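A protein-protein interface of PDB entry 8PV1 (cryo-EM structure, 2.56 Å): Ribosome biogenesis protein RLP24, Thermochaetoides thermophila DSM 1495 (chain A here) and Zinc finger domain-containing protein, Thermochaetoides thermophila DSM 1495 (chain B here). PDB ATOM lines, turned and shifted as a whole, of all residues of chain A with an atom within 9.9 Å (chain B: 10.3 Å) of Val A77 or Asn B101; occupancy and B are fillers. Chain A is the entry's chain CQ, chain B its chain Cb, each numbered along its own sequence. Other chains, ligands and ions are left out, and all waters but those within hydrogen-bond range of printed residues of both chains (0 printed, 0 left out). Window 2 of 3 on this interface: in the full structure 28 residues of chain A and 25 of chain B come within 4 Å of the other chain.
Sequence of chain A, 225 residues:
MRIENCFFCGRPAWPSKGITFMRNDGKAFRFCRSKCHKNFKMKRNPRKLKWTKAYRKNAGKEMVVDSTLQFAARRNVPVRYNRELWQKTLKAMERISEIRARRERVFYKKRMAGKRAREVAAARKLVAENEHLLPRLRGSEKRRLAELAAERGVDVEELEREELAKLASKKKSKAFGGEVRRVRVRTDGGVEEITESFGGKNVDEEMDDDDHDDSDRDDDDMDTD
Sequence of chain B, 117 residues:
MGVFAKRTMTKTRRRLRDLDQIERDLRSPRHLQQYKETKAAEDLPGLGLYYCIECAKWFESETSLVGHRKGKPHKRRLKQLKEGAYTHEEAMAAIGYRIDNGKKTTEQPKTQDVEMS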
ATOM      1  N   ALA A  73      12.368  14.695 -25.883  1.00  0.00           N
ATOM      2  CA  ALA A  73      12.193  13.310 -25.475  1.00  0.00           C
ATOM      3  C   ALA A  73      13.448  12.843 -24.756  1.00  0.00           C
ATOM      4  O   ALA A  73      14.515  13.450 -24.866  1.00  0.00           O
ATOM      5  CB  ALA A  73      11.898  12.402 -26.672  1.00  0.00           C
ATOM      6  N   ARG A  74      13.302  11.753 -24.008  1.00  0.00           N
ATOM      7  CA  ARG A  74      14.442  11.087 -23.391  1.00  0.00           C
ATOM      8  C   ARG A  74      15.101  10.206 -24.443  1.00  0.00           C
ATOM      9  O   ARG A  74      14.554   9.165 -24.820  1.00  0.00           O
ATOM     10  CB  ARG A  74      13.996  10.274 -22.179  1.00  0.00           C
ATOM     11  CG  ARG A  74      15.104   9.484 -21.503  1.00  0.00           C
ATOM     12  CD  ARG A  74      14.640   8.948 -20.155  1.00  0.00           C
ATOM     13  NE  ARG A  74      15.594   8.025 -19.551  1.00  0.00           N
ATOM     14  CZ  ARG A  74      16.680   8.394 -18.886  1.00  0.00           C
ATOM     15  NH1 ARG A  74      16.996   9.668 -18.725  1.00  0.00           N
ATOM     16  NH2 ARG A  74      17.470   7.459 -18.365  1.00  0.00           N
ATOM     17  N   ARG A  75      16.266  10.624 -24.929  1.00  0.00           N
ATOM     18  CA  ARG A  75      16.932   9.951 -26.038  1.00  0.00           C
ATOM     19  C   ARG A  75      17.783   8.813 -25.489  1.00  0.00           C
ATOM     20  O   ARG A  75      18.839   9.047 -24.895  1.00  0.00           O
ATOM     21  CB  ARG A  75      17.779  10.936 -26.837  1.00  0.00           C
ATOM     22  CG  ARG A  75      17.037  12.190 -27.233  1.00  0.00           C
ATOM     23  CD  ARG A  75      16.102  11.944 -28.396  1.00  0.00           C
ATOM     24  NE  ARG A  75      15.281  13.115 -28.672  1.00  0.00           N
ATOM     25  CZ  ARG A  75      14.564  13.287 -29.772  1.00  0.00           C
ATOM     26  NH1 ARG A  75      14.556  12.386 -30.740  1.00  0.00           N
ATOM     27  NH2 ARG A  75      13.835  14.392 -29.906  1.00  0.00           N
ATOM     28  N   ASN A  76      17.326   7.582 -25.700  1.00  0.00           N
ATOM     29  CA  ASN A  76      18.022   6.403 -25.214  1.00  0.00           C
ATOM     30  C   ASN A  76      19.001   5.824 -26.225  1.00  0.00           C
ATOM     31  O   ASN A  76      19.733   4.891 -25.886  1.00  0.00           O
ATOM     32  CB  ASN A  76      17.009   5.333 -24.806  1.00  0.00           C
ATOM     33  CG  ASN A  76      16.355   5.635 -23.476  1.00  0.00           C
ATOM     34  OD1 ASN A  76      16.891   6.388 -22.668  1.00  0.00           O
ATOM     35  ND2 ASN A  76      15.194   5.045 -23.240  1.00  0.00           N
ATOM     36  N   VAL A  77      19.034   6.348 -27.445  1.00  0.00           N
ATOM     37  CA  VAL A  77      20.040   5.970 -28.433  1.00  0.00           C
ATOM     38  C   VAL A  77      20.915   7.190 -28.696  1.00  0.00           C
ATOM     39  O   VAL A  77      20.448   8.164 -29.302  1.00  0.00           O
ATOM     40  CB  VAL A  77      19.395   5.448 -29.726  1.00  0.00           C
ATOM     41  CG1 VAL A  77      20.466   5.036 -30.720  1.00  0.00           C
ATOM     42  CG2 VAL A  77      18.475   4.285 -29.420  1.00  0.00           C
ATOM     43  N   PRO A  78      22.168   7.190 -28.244  1.00  0.00           N
ATOM     44  CA  PRO A  78      23.004   8.387 -28.386  1.00  0.00           C
ATOM     45  C   PRO A  78      23.411   8.648 -29.828  1.00  0.00           C
ATOM     46  O   PRO A  78      23.515   7.735 -30.648  1.00  0.00           O
ATOM     47  CB  PRO A  78      24.224   8.069 -27.514  1.00  0.00           C
ATOM     48  CG  PRO A  78      24.270   6.584 -27.467  1.00  0.00           C
ATOM     49  CD  PRO A  78      22.844   6.133 -27.476  1.00  0.00           C
ATOM     50  N   VAL A  79      23.642   9.923 -30.123  1.00  0.00           N
ATOM     51  CA  VAL A  79      24.084  10.386 -31.431  1.00  0.00           C
ATOM     52  C   VAL A  79      25.523  10.863 -31.300  1.00  0.00           C
ATOM     53  O   VAL A  79      25.879  11.513 -30.310  1.00  0.00           O
ATOM     54  CB  VAL A  79      23.161  11.505 -31.959  1.00  0.00           C
ATOM     55  CG1 VAL A  79      23.645  12.043 -33.300  1.00  0.00           C
ATOM     56  CG2 VAL A  79      21.737  10.997 -32.077  1.00  0.00           C
ATOM     57  N   ARG A  80      26.358  10.498 -32.274  1.00  0.00           N
ATOM     58  CA  ARG A  80      27.737  10.971 -32.311  1.00  0.00           C
ATOM     59  C   ARG A  80      27.770  12.491 -32.433  1.00  0.00           C
ATOM     60  O   ARG A  80      26.943  13.090 -33.127  1.00  0.00           O
ATOM     61  CB  ARG A  80      28.479  10.325 -33.481  1.00  0.00           C
ATOM     62  CG  ARG A  80      29.963  10.636 -33.545  1.00  0.00           C
ATOM     63  CD  ARG A  80      30.660   9.767 -34.577  1.00  0.00           C
ATOM     64  NE  ARG A  80      30.402   8.348 -34.362  1.00  0.00           N
ATOM     65  CZ  ARG A  80      31.114   7.569 -33.560  1.00  0.00           C
ATOM     66  NH1 ARG A  80      32.134   8.042 -32.862  1.00  0.00           N
ATOM     67  NH2 ARG A  80      30.793   6.285 -33.450  1.00  0.00           N
ATOM     68  N   LEU A  85      25.191  19.926 -36.102  1.00  0.00           N
ATOM     69  CA  LEU A  85      23.952  19.351 -35.591  1.00  0.00           C
ATOM     70  C   LEU A  85      23.546  19.998 -34.272  1.00  0.00           C
ATOM     71  O   LEU A  85      22.373  20.335 -34.080  1.00  0.00           O
ATOM     72  CB  LEU A  85      24.101  17.838 -35.433  1.00  0.00           C
ATOM     73  CG  LEU A  85      22.924  17.108 -34.783  1.00  0.00           C
ATOM     74  CD1 LEU A  85      21.682  17.232 -35.649  1.00  0.00           C
ATOM     75  CD2 LEU A  85      23.265  15.648 -34.540  1.00  0.00           C
ATOM     76  N   TRP A  86      24.506  20.215 -33.368  1.00  0.00           N
ATOM     77  CA  TRP A  86      24.199  20.919 -32.121  1.00  0.00           C
ATOM     78  C   TRP A  86      23.793  22.375 -32.357  1.00  0.00           C
ATOM     79  O   TRP A  86      22.877  22.878 -31.690  1.00  0.00           O
ATOM     80  CB  TRP A  86      25.379  20.815 -31.152  1.00  0.00           C
ATOM     81  CG  TRP A  86      25.204  19.737 -30.109  1.00  0.00           C
ATOM     82  CD1 TRP A  86      24.865  19.926 -28.802  1.00  0.00           C
ATOM     83  CD2 TRP A  86      25.265  18.318 -30.301  1.00  0.00           C
ATOM     84  NE1 TRP A  86      24.761  18.721 -28.156  1.00  0.00           N
ATOM     85  CE2 TRP A  86      24.997  17.717 -29.056  1.00  0.00           C
ATOM     86  CE3 TRP A  86      25.534  17.499 -31.398  1.00  0.00           C
ATOM     87  CZ2 TRP A  86      24.993  16.338 -28.880  1.00  0.00           C
ATOM     88  CZ3 TRP A  86      25.530  16.131 -31.221  1.00  0.00           C
ATOM     89  CH2 TRP A  86      25.263  15.564 -29.972  1.00  0.00           C
ATOM     90  N   MET B  92       5.140  11.874 -16.844  1.00  0.00           N
ATOM     91  CA  MET B  92       5.690  12.331 -18.118  1.00  0.00           C
ATOM     92  C   MET B  92       4.598  12.844 -19.047  1.00  0.00           C
ATOM     93  O   MET B  92       4.803  13.821 -19.776  1.00  0.00           O
ATOM     94  CB  MET B  92       6.477  11.211 -18.795  1.00  0.00           C
ATOM     95  CG  MET B  92       7.735  10.797 -18.068  1.00  0.00           C
ATOM     96  SD  MET B  92       8.626   9.522 -18.973  1.00  0.00           S
ATOM     97  CE  MET B  92       7.580   8.106 -18.659  1.00  0.00           C
ATOM     98  N   ARG B  98       8.279  12.295 -23.260  1.00  0.00           N
ATOM     99  CA  ARG B  98       8.187  10.925 -23.744  1.00  0.00           C
ATOM    100  C   ARG B  98       9.571  10.293 -23.747  1.00  0.00           C
ATOM    101  O   ARG B  98      10.585  10.954 -23.511  1.00  0.00           O
ATOM    102  CB  ARG B  98       7.571  10.859 -25.147  1.00  0.00           C
ATOM    103  CG  ARG B  98       8.213  11.801 -26.143  1.00  0.00           C
ATOM    104  CD  ARG B  98       7.818  11.461 -27.565  1.00  0.00           C
ATOM    105  NE  ARG B  98       8.456  12.348 -28.529  1.00  0.00           N
ATOM    106  CZ  ARG B  98       9.262  11.945 -29.501  1.00  0.00           C
ATOM    107  NH1 ARG B  98       9.547  10.665 -29.675  1.00  0.00           N
ATOM    108  NH2 ARG B  98       9.795  12.847 -30.318  1.00  0.00           N
ATOM    109  N   ILE B  99       9.599   8.993 -24.022  1.00  0.00           N
ATOM    110  CA  ILE B  99      10.832   8.220 -24.109  1.00  0.00           C
ATOM    111  C   ILE B  99      11.043   7.843 -25.568  1.00  0.00           C
ATOM    112  O   ILE B  99      10.135   7.310 -26.217  1.00  0.00           O
ATOM    113  CB  ILE B  99      10.784   6.970 -23.217  1.00  0.00           C
ATOM    114  CG1 ILE B  99      10.710   7.362 -21.743  1.00  0.00           C
ATOM    115  CG2 ILE B  99      11.992   6.089 -23.452  1.00  0.00           C
ATOM    116  CD1 ILE B  99       9.982   6.354 -20.894  1.00  0.00           C
ATOM    117  N   ASP B 100      12.233   8.127 -26.085  1.00  0.00           N
ATOM    118  CA  ASP B 100      12.616   7.743 -27.436  1.00  0.00           C
ATOM    119  C   ASP B 100      13.562   6.552 -27.357  1.00  0.00           C
ATOM    120  O   ASP B 100      14.716   6.696 -26.942  1.00  0.00           O
ATOM    121  CB  ASP B 100      13.274   8.910 -28.169  1.00  0.00           C
ATOM    122  CG  ASP B 100      13.776   8.523 -29.542  1.00  0.00           C
ATOM    123  OD1 ASP B 100      13.065   7.776 -30.245  1.00  0.00           O
ATOM    124  OD2 ASP B 100      14.883   8.963 -29.918  1.00  0.00           O
ATOM    125  N   ASN B 101      13.071   5.379 -27.755  1.00  0.00           N
ATOM    126  CA  ASN B 101      13.856   4.151 -27.744  1.00  0.00           C
ATOM    127  C   ASN B 101      14.400   3.800 -29.123  1.00  0.00           C
ATOM    128  O   ASN B 101      14.953   2.713 -29.310  1.00  0.00           O
ATOM    129  CB  ASN B 101      13.021   2.995 -27.196  1.00  0.00           C
ATOM    130  CG  ASN B 101      12.972   2.977 -25.684  1.00  0.00           C
ATOM    131  OD1 ASN B 101      13.991   2.791 -25.021  1.00  0.00           O
ATOM    132  ND2 ASN B 101      11.784   3.176 -25.129  1.00  0.00           N
ATOM    133  N   GLY B 102      14.254   4.697 -30.092  1.00  0.00           N
ATOM    134  CA  GLY B 102      14.729   4.448 -31.440  1.00  0.00           C
ATOM    135  C   GLY B 102      13.665   3.861 -32.344  1.00  0.00           C
ATOM    136  O   GLY B 102      13.315   4.447 -33.367  1.00  0.00           O
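Among the printed residues, merely in contact across the chains: Ala A73 with Arg B98, Arg A74 with Ile B99, Asn A76 with Ile B99 and Val A77 with Asn B101.
Printed residues of chain B within 4 Å of Ala A73: Arg B98 (3.5 Å).
Of the printed residues of chain B, Arg A74 touches Arg B98, Ile B99 and Asp B100.
Printed residues of chain B within 4 Å of Arg A75: Asp B100 (3.5 Å).
Of the printed residues of chain A, Arg B98 touches Ala A73 (3.5 Å) and Arg A74 (2.9 Å).
Of the printed residues of chain A, Ile B99 touches Arg A74 and Asn A76.
Of chain A, only Arg A74 (2.8 Å), Arg A75 (3.5 Å) and Asn A76 (3.0 Å) come within 4 Å of Asp B100.
Of chain A, only Asn A76 (3.1 Å) and Val A77 (3.9 Å) come within 4 Å of Asn B101.
No residue of chain A comes within 4 Å of Gly B102.
The backbone carbonyl oxygen of Arg A74 is in hydrogen-bond range of the backbone NH of Asp B100, at 2.8 Å.
O of Arg B98 sits at hydrogen-bond distance from N of Arg A74 (2.9 Å).
The side-chain amide nitrogen (ND2) of Asn A76 is in hydrogen-bond range of the side-chain amide oxygen (OD1) of Asn B101.
The guanidinium group (NH1) of Arg A75 lies within salt-bridge range of the side-chain carboxylate (OD2) of Asp B100.
O of Asp B100 is in hydrogen-bond range of N of Asn A76 (3.0 Å).
Of the 10 printed residues of chain A, 5 touch a printed residue of chain B.
Printed residues of chain A that touch a printed residue of chain B: Ala A73, Arg A74, Arg A75, Asn A76 and Val A77.
Of the 6 printed residues of chain B, 4 touch a printed residue of chain A.
Printed residues of chain B that touch a printed residue of chain A: Arg B98, Ile B99, Asp B100 and Asn B101.
Among the printed residues, 9 pairs touch across the chains.
Among the printed residues, Asp or Glu carboxylates within 4 Å of a Lys or Arg side-chain nitrogen of the other chain: Arg A75 with Asp B100 (3.5 Å).
The backbone NH of Gly B102 lies within hydrogen-bond range of the side-chain carboxylate of Asp B100, 3.3 Å away.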
